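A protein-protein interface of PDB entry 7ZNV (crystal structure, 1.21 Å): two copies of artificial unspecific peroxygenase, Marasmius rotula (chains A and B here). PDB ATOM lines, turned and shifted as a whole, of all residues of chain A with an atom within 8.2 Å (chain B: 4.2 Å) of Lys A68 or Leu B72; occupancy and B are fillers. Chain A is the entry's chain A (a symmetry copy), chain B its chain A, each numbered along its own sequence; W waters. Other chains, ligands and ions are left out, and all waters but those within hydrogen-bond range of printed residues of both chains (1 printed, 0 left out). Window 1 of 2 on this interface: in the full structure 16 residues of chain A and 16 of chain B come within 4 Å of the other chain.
O of Leu A71 lies within hydrogen-bond range of NZ of Lys B68. O of Ser A74 lies within hydrogen-bond range of NZ of Lys B68 (2.8 Å). The backbone carbonyl oxygen of Leu B71 sits at hydrogen-bond distance from the side-chain amino group of Lys A68 (2.9 Å). The backbone carbonyl oxygen of Ser B74 sits at hydrogen-bond distance from the side-chain amino group of Lys A68 (2.8 Å). The backbone carbonyl oxygen (O) of Glu B76 sits at hydrogen-bond distance from the side-chain amino group (NZ) of Lys A68.
The side-chain hydroxyl (OG) of Ser B74 sits at hydrogen-bond distance from the backbone NH (N) of Glu B76 (3.0 Å).
Ile A45 touches Leu B71. Pro B77 touches Ile A45 (O to CG2, 3.3 Å). CG2 of Ile A64 touches O of Glu B76 (3.8 Å). CG2 of Ile A64 touches CA of Pro B77, at 3.8 Å. Leu A65 touches Leu B72. Leu B72 touches Lys A68 (CD2 to CB, 3.9 Å). Pro B77 touches Lys A68 (O to CE, 3.3 Å). Leu A72 touches Lys B68 (CD2 to CB, 3.9 Å). Ile A235 touches Leu B237 (CD1 to CD2, 3.8 Å). Leu A237 touches Ile B235.
Of chain B, only Leu B71, Leu B72, Ser B74, Glu B76 and Pro B77 come within 4 Å of Lys A68. Leu B72 touches two residues of chain A. Of the printed residues of chain B, Ser A74 touches Lys B68 (2.8 Å). Of the printed residues of chain B, Leu A71 touches Lys B68 (2.9 Å). Printed residues of chain A within 4 Å of Pro B77: Ile A45, Ile A64 and Lys A68. Of the printed residues of chain B, Leu A72 touches Lys B68. Of the printed residues of chain B, Ile A45 touches Leu B71 (3.9 Å) and Pro B77 (3.3 Å). Leu A85 touches none of the printed residues of chain B. Asp A61 touches none of the printed residues of chain B. The nearest printed residue of chain B that does not touch Lys A68 is Lys B68 (5.0 Å). The nearest residue of chain A that does not touch Leu B72 is Val A69 (4.3 Å). The nearest printed residue of chain A that does not touch Glu B76 is Ile A45 (6.1 Å).
Of the 13 printed residues of chain B, 8 touch a printed residue of chain A. Printed residues of chain B that touch a printed residue of chain A: Lys B68, Leu B71, Leu B72, Ser B74, Glu B76, Pro B77, Ile B235 and Leu B237. Among the printed residues, 16 pairs touch across the chains. Among the printed residues, no Asp or Glu carboxylate lies within 4 Å of a Lys or Arg side-chain nitrogen of the other chain.
Lys A68 touches Leu B71, and with the chains exchanged Leu A71 touches Lys B68. Lys A68 touches Leu B72, and with the chains exchanged Leu A72 touches Lys B68. Lys A68 touches Ser B74, and with the chains exchanged Ser A74 touches Lys B68. Ile A235 touches Leu B237, and with the chains exchanged Leu A237 touches Ile B235. Positions printed for both chains: 68, 69, 70, 71, 72, 73, 74, 235 and 237.
Water W1 bridges the backbone carbonyl oxygen (O) of Lys A68 (2.9 Å) and the backbone carbonyl oxygen (O) of Lys B68 (2.9 Å).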
ATOM      1  N   THR A  44     -17.584  20.749   8.741  1.00  0.00           N
ATOM      2  CA  THR A  44     -16.687  19.900   9.518  1.00  0.00           C
ATOM      3  C   THR A  44     -16.162  20.647  10.759  1.00  0.00           C
ATOM      4  O   THR A  44     -16.259  21.868  10.860  1.00  0.00           O
ATOM      5  CB  THR A  44     -15.478  19.467   8.678  1.00  0.00           C
ATOM      6  OG1 THR A  44     -14.757  20.671   8.408  1.00  0.00           O
ATOM      7  CG2 THR A  44     -15.879  18.739   7.418  1.00  0.00           C
ATOM      8  N   ILE A  45     -15.560  19.909  11.670  1.00  0.00           N
ATOM      9  CA  ILE A  45     -14.922  20.531  12.834  1.00  0.00           C
ATOM     10  C   ILE A  45     -13.854  21.533  12.421  1.00  0.00           C
ATOM     11  O   ILE A  45     -13.867  22.671  12.891  1.00  0.00           O
ATOM     12  CB  ILE A  45     -14.401  19.487  13.829  1.00  0.00           C
ATOM     13  CG1 ILE A  45     -15.553  18.613  14.378  1.00  0.00           C
ATOM     14  CG2 ILE A  45     -13.588  20.151  14.903  1.00  0.00           C
ATOM     15  CD1 ILE A  45     -15.034  17.308  14.931  1.00  0.00           C
ATOM     16  N   ILE A  48     -15.399  24.842  11.447  1.00  0.00           N
ATOM     17  CA  ILE A  48     -15.866  25.635  12.597  1.00  0.00           C
ATOM     18  C   ILE A  48     -14.666  26.337  13.227  1.00  0.00           C
ATOM     19  O   ILE A  48     -14.739  27.525  13.564  1.00  0.00           O
ATOM     20  CB  ILE A  48     -16.529  24.704  13.634  1.00  0.00           C
ATOM     21  CG1 ILE A  48     -17.859  24.174  13.093  1.00  0.00           C
ATOM     22  CG2 ILE A  48     -16.639  25.428  14.969  1.00  0.00           C
ATOM     23  CD1 ILE A  48     -18.970  25.174  13.087  1.00  0.00           C
ATOM     24  N   VAL A  49     -13.564  25.598  13.441  1.00  0.00           N
ATOM     25  CA  VAL A  49     -12.394  26.171  14.123  1.00  0.00           C
ATOM     26  C   VAL A  49     -11.834  27.351  13.308  1.00  0.00           C
ATOM     27  O   VAL A  49     -11.577  28.400  13.888  1.00  0.00           O
ATOM     28  CB  VAL A  49     -11.332  25.070  14.313  1.00  0.00           C
ATOM     29  CG1 VAL A  49     -10.018  25.678  14.787  1.00  0.00           C
ATOM     30  CG2 VAL A  49     -11.838  24.012  15.294  1.00  0.00           C
ATOM     31  N   ASP A  61      -9.676  25.581  21.388  1.00  0.00           N
ATOM     32  CA  ASP A  61     -10.149  24.473  22.275  1.00  0.00           C
ATOM     33  C   ASP A  61     -11.678  24.384  22.424  1.00  0.00           C
ATOM     34  O   ASP A  61     -12.285  23.264  22.343  1.00  0.00           O
ATOM     35  CB  ASP A  61      -9.466  24.556  23.635  1.00  0.00           C
ATOM     36  CG  ASP A  61      -9.579  25.873  24.378  1.00  0.00           C
ATOM     37  OD1 ASP A  61     -10.427  26.702  23.995  1.00  0.00           O
ATOM     38  OD2 ASP A  61      -8.833  26.048  25.379  1.00  0.00           O
ATOM     39  N   ILE A  62     -12.362  25.494  22.522  1.00  0.00           N
ATOM     40  CA  ILE A  62     -13.715  25.495  22.959  1.00  0.00           C
ATOM     41  C   ILE A  62     -14.625  25.220  21.685  1.00  0.00           C
ATOM     42  O   ILE A  62     -15.662  24.474  21.619  1.00  0.00           O
ATOM     43  CB  ILE A  62     -14.016  26.887  23.539  1.00  0.00           C
ATOM     44  CG1 ILE A  62     -15.488  27.005  23.940  1.00  0.00           C
ATOM     45  CG2 ILE A  62     -13.609  28.010  22.601  1.00  0.00           C
ATOM     46  CD1 ILE A  62     -15.920  25.991  24.967  1.00  0.00           C
ATOM     47  N   LEU A  63     -14.031  25.748  20.614  1.00  0.00           N
ATOM     48  CA  LEU A  63     -14.727  25.450  19.394  1.00  0.00           C
ATOM     49  C   LEU A  63     -14.685  23.956  19.090  1.00  0.00           C
ATOM     50  O   LEU A  63     -15.634  23.442  18.563  1.00  0.00           O
ATOM     51  CB  LEU A  63     -14.106  26.243  18.276  1.00  0.00           C
ATOM     52  CG  LEU A  63     -14.219  27.753  18.385  1.00  0.00           C
ATOM     53  CD1 LEU A  63     -13.478  28.423  17.201  1.00  0.00           C
ATOM     54  CD2 LEU A  63     -15.675  28.195  18.426  1.00  0.00           C
ATOM     55  N   ILE A  64     -13.515  23.330  19.301  1.00  0.00           N
ATOM     56  CA  ILE A  64     -13.391  21.882  19.006  1.00  0.00           C
ATOM     57  C   ILE A  64     -14.391  21.067  19.829  1.00  0.00           C
ATOM     58  O   ILE A  64     -15.078  20.226  19.265  1.00  0.00           O
ATOM     59  CB  ILE A  64     -11.952  21.415  19.226  1.00  0.00           C
ATOM     60  CG1 ILE A  64     -10.978  22.029  18.231  1.00  0.00           C
ATOM     61  CG2 ILE A  64     -11.860  19.894  19.218  1.00  0.00           C
ATOM     62  CD1 ILE A  64      -9.518  21.846  18.588  1.00  0.00           C
ATOM     63  N   LEU A  65     -14.529  21.301  21.104  1.00  0.00           N
ATOM     64  CA  LEU A  65     -15.420  20.499  21.911  1.00  0.00           C
ATOM     65  C   LEU A  65     -16.847  20.699  21.464  1.00  0.00           C
ATOM     66  O   LEU A  65     -17.633  19.773  21.317  1.00  0.00           O
ATOM     67  CB  LEU A  65     -15.211  20.871  23.373  1.00  0.00           C
ATOM     68  CG  LEU A  65     -16.210  20.196  24.298  1.00  0.00           C
ATOM     69  CD1 LEU A  65     -16.169  18.675  24.208  1.00  0.00           C
ATOM     70  CD2 LEU A  65     -15.954  20.669  25.737  1.00  0.00           C
ATOM     71  N   ALA A  66     -17.283  21.969  21.325  1.00  0.00           N
ATOM     72  CA  ALA A  66     -18.640  22.279  20.862  1.00  0.00           C
ATOM     73  C   ALA A  66     -18.942  21.609  19.527  1.00  0.00           C
ATOM     74  O   ALA A  66     -20.014  21.096  19.336  1.00  0.00           O
ATOM     75  CB  ALA A  66     -18.849  23.773  20.801  1.00  0.00           C
ATOM     76  N   ALA A  67     -17.969  21.682  18.605  1.00  0.00           N
ATOM     77  CA  ALA A  67     -18.182  21.098  17.298  1.00  0.00           C
ATOM     78  C   ALA A  67     -18.278  19.561  17.346  1.00  0.00           C
ATOM     79  O   ALA A  67     -19.075  18.987  16.637  1.00  0.00           O
ATOM     80  CB  ALA A  67     -17.113  21.517  16.322  1.00  0.00           C
ATOM     81  N   LYS A  68     -17.453  18.950  18.179  1.00  0.00           N
ATOM     82  CA  LYS A  68     -17.550  17.474  18.364  1.00  0.00           C
ATOM     83  C   LYS A  68     -18.921  17.107  18.899  1.00  0.00           C
ATOM     84  O   LYS A  68     -19.499  16.110  18.467  1.00  0.00           O
ATOM     85  CB  LYS A  68     -16.456  17.004  19.316  1.00  0.00           C
ATOM     86  CG  LYS A  68     -15.078  16.948  18.681  1.00  0.00           C
ATOM     87  CD  LYS A  68     -14.018  16.624  19.686  1.00  0.00           C
ATOM     88  CE  LYS A  68     -12.626  16.611  19.084  1.00  0.00           C
ATOM     89  NZ  LYS A  68     -11.581  16.491  20.105  1.00  0.00           N
ATOM     90  N   VAL A  69     -19.437  17.853  19.858  1.00  0.00           N
ATOM     91  CA  VAL A  69     -20.775  17.579  20.400  1.00  0.00           C
ATOM     92  C   VAL A  69     -21.800  17.849  19.293  1.00  0.00           C
ATOM     93  O   VAL A  69     -22.780  17.141  19.143  1.00  0.00           O
ATOM     94  CB  VAL A  69     -20.994  18.358  21.696  1.00  0.00           C
ATOM     95  CG1 VAL A  69     -22.462  18.278  22.147  1.00  0.00           C
ATOM     96  CG2 VAL A  69     -20.042  17.852  22.780  1.00  0.00           C
ATOM     97  N   GLY A  70     -21.620  18.939  18.538  1.00  0.00           N
ATOM     98  CA  GLY A  70     -22.528  19.243  17.467  1.00  0.00           C
ATOM     99  C   GLY A  70     -22.631  18.126  16.457  1.00  0.00           C
ATOM    100  O   GLY A  70     -23.712  17.924  15.875  1.00  0.00           O
ATOM    101  N   LEU A  71     -21.536  17.405  16.195  1.00  0.00           N
ATOM    102  CA  LEU A  71     -21.623  16.271  15.245  1.00  0.00           C
ATOM    103  C   LEU A  71     -22.651  15.225  15.682  1.00  0.00           C
ATOM    104  O   LEU A  71     -23.192  14.531  14.819  1.00  0.00           O
ATOM    105  CB  LEU A  71     -20.261  15.591  15.102  1.00  0.00           C
ATOM    106  CG  LEU A  71     -19.250  16.250  14.176  1.00  0.00           C
ATOM    107  CD1 LEU A  71     -18.016  15.370  14.143  1.00  0.00           C
ATOM    108  CD2 LEU A  71     -19.796  16.405  12.779  1.00  0.00           C
ATOM    109  N   LEU A  72     -22.928  15.132  16.993  1.00  0.00           N
ATOM    110  CA  LEU A  72     -23.914  14.153  17.472  1.00  0.00           C
ATOM    111  C   LEU A  72     -25.285  14.445  16.915  1.00  0.00           C
ATOM    112  O   LEU A  72     -26.156  13.559  16.881  1.00  0.00           O
ATOM    113  CB  LEU A  72     -23.924  14.103  18.992  1.00  0.00           C
ATOM    114  CG  LEU A  72     -22.626  13.663  19.614  1.00  0.00           C
ATOM    115  CD1 LEU A  72     -22.614  13.917  21.097  1.00  0.00           C
ATOM    116  CD2 LEU A  72     -22.333  12.187  19.316  1.00  0.00           C
ATOM    117  N   THR A  73     -25.562  15.689  16.556  1.00  0.00           N
ATOM    118  CA  THR A  73     -26.887  16.094  16.042  1.00  0.00           C
ATOM    119  C   THR A  73     -27.109  15.666  14.607  1.00  0.00           C
ATOM    120  O   THR A  73     -28.242  15.783  14.124  1.00  0.00           O
ATOM    121  CB  THR A  73     -27.140  17.590  16.198  1.00  0.00           C
ATOM    122  OG1 THR A  73     -26.365  18.316  15.219  1.00  0.00           O
ATOM    123  CG2 THR A  73     -26.904  18.089  17.581  1.00  0.00           C
ATOM    124  N   SER A  74     -26.075  15.166  13.957  1.00  0.00           N
ATOM    125  CA  SER A  74     -26.085  14.872  12.526  1.00  0.00           C
ATOM    126  C   SER A  74     -25.987  13.376  12.305  1.00  0.00           C
ATOM    127  O   SER A  74     -25.237  12.710  12.989  1.00  0.00           O
ATOM    128  CB  SER A  74     -24.917  15.545  11.908  1.00  0.00           C
ATOM    129  OG  SER A  74     -24.715  15.093  10.564  1.00  0.00           O
ATOM    130  N   PHE A  80     -21.992  18.319  10.025  1.00  0.00           N
ATOM    131  CA  PHE A  80     -23.356  18.692  10.358  1.00  0.00           C
ATOM    132  C   PHE A  80     -23.779  19.841   9.476  1.00  0.00           C
ATOM    133  O   PHE A  80     -22.943  20.527   8.867  1.00  0.00           O
ATOM    134  CB  PHE A  80     -23.548  19.031  11.835  1.00  0.00           C
ATOM    135  CG  PHE A  80     -22.647  20.084  12.428  1.00  0.00           C
ATOM    136  CD1 PHE A  80     -22.818  21.413  12.120  1.00  0.00           C
ATOM    137  CD2 PHE A  80     -21.686  19.768  13.369  1.00  0.00           C
ATOM    138  CE1 PHE A  80     -21.982  22.378  12.675  1.00  0.00           C
ATOM    139  CE2 PHE A  80     -20.870  20.719  13.939  1.00  0.00           C
ATOM    140  CZ  PHE A  80     -21.003  22.031  13.567  1.00  0.00           C
ATOM    141  N   LEU A  85     -28.183  21.418  14.418  1.00  0.00           N
ATOM    142  CA  LEU A  85     -27.828  21.858  15.765  1.00  0.00           C
ATOM    143  C   LEU A  85     -29.047  22.270  16.570  1.00  0.00           C
ATOM    144  O   LEU A  85     -28.880  22.502  17.789  1.00  0.00           O
ATOM    145  CB  LEU A  85     -26.848  23.023  15.679  1.00  0.00           C
ATOM    146  CG  LEU A  85     -25.505  22.742  15.017  1.00  0.00           C
ATOM    147  CD1 LEU A  85     -24.695  24.028  14.932  1.00  0.00           C
ATOM    148  CD2 LEU A  85     -24.733  21.661  15.732  1.00  0.00           C
ATOM    149  N   THR A  90     -29.024  18.197  23.059  1.00  0.00           N
ATOM    150  CA  THR A  90     -27.603  17.978  22.757  1.00  0.00           C
ATOM    151  C   THR A  90     -26.860  19.200  23.245  1.00  0.00           C
ATOM    152  O   THR A  90     -26.239  19.156  24.319  1.00  0.00           O
ATOM    153  CB  THR A  90     -27.386  17.608  21.294  1.00  0.00           C
ATOM    154  OG1 THR A  90     -28.225  16.501  20.936  1.00  0.00           O
ATOM    155  CG2 THR A  90     -25.931  17.326  21.019  1.00  0.00           C
ATOM    156  N   ILE A  91     -26.963  20.292  22.486  1.00  0.00           N
ATOM    157  CA  ILE A  91     -26.496  21.611  22.977  1.00  0.00           C
ATOM    158  C   ILE A  91     -27.753  22.458  23.237  1.00  0.00           C
ATOM    159  O   ILE A  91     -27.835  23.083  24.280  1.00  0.00           O
ATOM    160  CB  ILE A  91     -25.575  22.311  21.959  1.00  0.00           C
ATOM    161  CG1 ILE A  91     -24.290  21.511  21.731  1.00  0.00           C
ATOM    162  CG2 ILE A  91     -25.287  23.740  22.394  1.00  0.00           C
ATOM    163  CD1 ILE A  91     -23.467  21.980  20.548  1.00  0.00           C
ATOM    164  N   ILE A 235     -26.283  14.623  27.408  1.00  0.00           N
ATOM    165  CA  ILE A 235     -26.192  15.056  26.002  1.00  0.00           C
ATOM    166  C   ILE A 235     -26.966  14.090  25.138  1.00  0.00           C
ATOM    167  O   ILE A 235     -26.523  12.929  24.989  1.00  0.00           O
ATOM    168  CB  ILE A 235     -24.730  15.184  25.593  1.00  0.00           C
ATOM    169  CG1 ILE A 235     -24.018  16.235  26.432  1.00  0.00           C
ATOM    170  CG2 ILE A 235     -24.648  15.519  24.115  1.00  0.00           C
ATOM    171  CD1 ILE A 235     -22.519  16.303  26.238  1.00  0.00           C
ATOM    172  N   LEU A 237     -27.827  11.951  22.183  1.00  0.00           N
ATOM    173  CA  LEU A 237     -26.747  11.405  21.328  1.00  0.00           C
ATOM    174  C   LEU A 237     -27.116  11.211  19.879  1.00  0.00           C
ATOM    175  O   LEU A 237     -26.175  10.939  19.088  1.00  0.00           O
ATOM    176  CB  LEU A 237     -26.267  10.064  21.861  1.00  0.00           C
ATOM    177  CG  LEU A 237     -25.572  10.154  23.208  1.00  0.00           C
ATOM    178  CD1 LEU A 237     -25.138   8.763  23.662  1.00  0.00           C
ATOM    179  CD2 LEU A 237     -24.391  11.097  23.196  1.00  0.00           C
ATOM    180  N   LYS B  68     -17.571   9.408  16.954  1.00  0.00           N
ATOM    181  CA  LYS B  68     -17.824  10.807  17.402  1.00  0.00           C
ATOM    182  C   LYS B  68     -17.574  10.928  18.893  1.00  0.00           C
ATOM    183  O   LYS B  68     -17.005  11.923  19.339  1.00  0.00           O
ATOM    184  CB  LYS B  68     -19.257  11.203  17.061  1.00  0.00           C
ATOM    185  CG  LYS B  68     -19.469  11.514  15.590  1.00  0.00           C
ATOM    186  CD  LYS B  68     -20.913  11.755  15.278  1.00  0.00           C
ATOM    187  CE  LYS B  68     -21.156  12.019  13.805  1.00  0.00           C
ATOM    188  NZ  LYS B  68     -22.584  12.056  13.476  1.00  0.00           N
ATOM    189  N   VAL B  69     -18.026   9.969  19.681  1.00  0.00           N
ATOM    190  CA  VAL B  69     -17.790  10.000  21.131  1.00  0.00           C
ATOM    191  C   VAL B  69     -16.286   9.836  21.371  1.00  0.00           C
ATOM    192  O   VAL B  69     -15.707  10.456  22.245  1.00  0.00           O
ATOM    193  CB  VAL B  69     -18.679   8.979  21.837  1.00  0.00           C
ATOM    194  CG1 VAL B  69     -18.278   8.826  23.313  1.00  0.00           C
ATOM    195  CG2 VAL B  69     -20.149   9.372  21.690  1.00  0.00           C
ATOM    196  N   GLY B  70     -15.638   8.927  20.632  1.00  0.00           N
ATOM    197  CA  GLY B  70     -14.223   8.736  20.786  1.00  0.00           C
ATOM    198  C   GLY B  70     -13.435  10.003  20.559  1.00  0.00           C
ATOM    199  O   GLY B  70     -12.389  10.197  21.203  1.00  0.00           O
ATOM    200  N   LEU B  71     -13.877  10.867  19.639  1.00  0.00           N
ATOM    201  CA  LEU B  71     -13.150  12.143  19.433  1.00  0.00           C
ATOM    202  C   LEU B  71     -13.070  12.979  20.711  1.00  0.00           C
ATOM    203  O   LEU B  71     -12.128  13.762  20.849  1.00  0.00           O
ATOM    204  CB  LEU B  71     -13.829  12.971  18.343  1.00  0.00           C
ATOM    205  CG  LEU B  71     -13.529  12.601  16.899  1.00  0.00           C
ATOM    206  CD1 LEU B  71     -14.252  13.592  16.010  1.00  0.00           C
ATOM    207  CD2 LEU B  71     -12.049  12.652  16.610  1.00  0.00           C
ATOM    208  N   LEU B  72     -14.029  12.801  21.634  1.00  0.00           N
ATOM    209  CA  LEU B  72     -14.002  13.569  22.887  1.00  0.00           C
ATOM    210  C   LEU B  72     -12.771  13.247  23.695  1.00  0.00           C
ATOM    211  O   LEU B  72     -12.365  14.030  24.570  1.00  0.00           O
ATOM    212  CB  LEU B  72     -15.276  13.338  23.686  1.00  0.00           C
ATOM    213  CG  LEU B  72     -16.537  13.786  22.998  1.00  0.00           C
ATOM    214  CD1 LEU B  72     -17.761  13.265  23.704  1.00  0.00           C
ATOM    215  CD2 LEU B  72     -16.595  15.313  22.872  1.00  0.00           C
ATOM    216  N   THR B  73     -12.194  12.068  23.514  1.00  0.00           N
ATOM    217  CA  THR B  73     -11.012  11.632  24.285  1.00  0.00           C
ATOM    218  C   THR B  73      -9.735  12.293  23.813  1.00  0.00           C
ATOM    219  O   THR B  73      -8.710  12.152  24.492  1.00  0.00           O
ATOM    220  CB  THR B  73     -10.855  10.115  24.303  1.00  0.00           C
ATOM    221  OG1 THR B  73     -10.376   9.666  23.017  1.00  0.00           O
ATOM    222  CG2 THR B  73     -12.089   9.397  24.723  1.00  0.00           C
ATOM    223  N   SER B  74      -9.795  13.005  22.704  1.00  0.00           N
ATOM    224  CA  SER B  74      -8.620  13.556  22.031  1.00  0.00           C
ATOM    225  C   SER B  74      -8.640  15.069  22.111  1.00  0.00           C
ATOM    226  O   SER B  74      -9.683  15.670  21.956  1.00  0.00           O
ATOM    227  CB  SER B  74      -8.660  13.130  20.612  1.00  0.00           C
ATOM    228  OG  SER B  74      -7.689  13.841  19.834  1.00  0.00           O
ATOM    229  N   GLU B  76      -7.229  16.827  19.796  1.00  0.00           N
ATOM    230  CA  GLU B  76      -7.143  17.262  18.397  1.00  0.00           C
ATOM    231  C   GLU B  76      -8.494  17.573  17.824  1.00  0.00           C
ATOM    232  O   GLU B  76      -9.540  17.067  18.274  1.00  0.00           O
ATOM    233  CB  GLU B  76      -6.445  16.196  17.580  1.00  0.00           C
ATOM    234  CG  GLU B  76      -4.988  16.013  17.974  1.00  0.00           C
ATOM    235  CD  GLU B  76      -4.151  17.281  17.809  1.00  0.00           C
ATOM    236  OE1 GLU B  76      -4.258  17.901  16.751  1.00  0.00           O
ATOM    237  OE2 GLU B  76      -3.473  17.653  18.788  1.00  0.00           O
ATOM    238  N   PRO B  77      -8.570  18.376  16.751  1.00  0.00           N
ATOM    239  CA  PRO B  77      -9.845  18.748  16.217  1.00  0.00           C
ATOM    240  C   PRO B  77     -10.690  17.591  15.704  1.00  0.00           C
ATOM    241  O   PRO B  77     -11.883  17.538  16.005  1.00  0.00           O
ATOM    242  CB  PRO B  77      -9.487  19.690  15.032  1.00  0.00           C
ATOM    243  CG  PRO B  77      -8.110  20.186  15.311  1.00  0.00           C
ATOM    244  CD  PRO B  77      -7.443  19.130  16.137  1.00  0.00           C
ATOM    245  N   ILE B 235     -21.009  11.040  29.892  1.00  0.00           N
ATOM    246  CA  ILE B 235     -19.835  10.886  29.013  1.00  0.00           C
ATOM    247  C   ILE B 235     -18.795  11.909  29.395  1.00  0.00           C
ATOM    248  O   ILE B 235     -19.026  13.117  29.161  1.00  0.00           O
ATOM    249  CB  ILE B 235     -20.264  10.984  27.555  1.00  0.00           C
ATOM    250  CG1 ILE B 235     -21.242   9.876  27.196  1.00  0.00           C
ATOM    251  CG2 ILE B 235     -19.035  10.937  26.665  1.00  0.00           C
ATOM    252  CD1 ILE B 235     -21.876   9.997  25.828  1.00  0.00           C
ATOM    253  N   LEU B 237     -16.075  14.457  28.992  1.00  0.00           N
ATOM    254  CA  LEU B 237     -15.994  15.258  27.748  1.00  0.00           C
ATOM    255  C   LEU B 237     -14.601  15.677  27.348  1.00  0.00           C
ATOM    256  O   LEU B 237     -14.471  16.184  26.203  1.00  0.00           O
ATOM    257  CB  LEU B 237     -16.834  16.520  27.866  1.00  0.00           C
ATOM    258  CG  LEU B 237     -18.326  16.256  27.960  1.00  0.00           C
ATOM    259  CD1 LEU B 237     -19.081  17.575  28.085  1.00  0.00           C
ATOM    260  CD2 LEU B 237     -18.853  15.455  26.791  1.00  0.00           C
ATOM    261  N   SER B 238     -13.624  15.465  28.175  1.00  0.00           N
ATOM    262  CA  SER B 238     -12.233  15.848  27.816  1.00  0.00           C
ATOM    263  C   SER B 238     -11.257  15.067  28.648  1.00  0.00           C
ATOM    264  O   SER B 238     -11.569  14.692  29.776  1.00  0.00           O
ATOM    265  CB  SER B 238     -12.103  17.339  28.090  1.00  0.00           C
ATOM    266  OG  SER B 238     -10.741  17.758  28.131  1.00  0.00           O
ATOM    267  N   PRO B 239     -10.012  14.863  28.170  1.00  0.00           N
ATOM    268  CA  PRO B 239      -9.014  14.268  29.021  1.00  0.00           C
ATOM    269  C   PRO B 239      -8.296  15.397  29.773  1.00  0.00           C
ATOM    270  O   PRO B 239      -7.282  15.102  30.378  1.00  0.00           O
ATOM    271  CB  PRO B 239      -8.069  13.600  28.015  1.00  0.00           C
ATOM    272  CG  PRO B 239      -8.101  14.526  26.821  1.00  0.00           C
ATOM    273  CD  PRO B 239      -9.505  15.096  26.803  1.00  0.00           C
HETATM  274  O   HOH W   1     -17.532  14.175  17.602  1.00  0.00           O
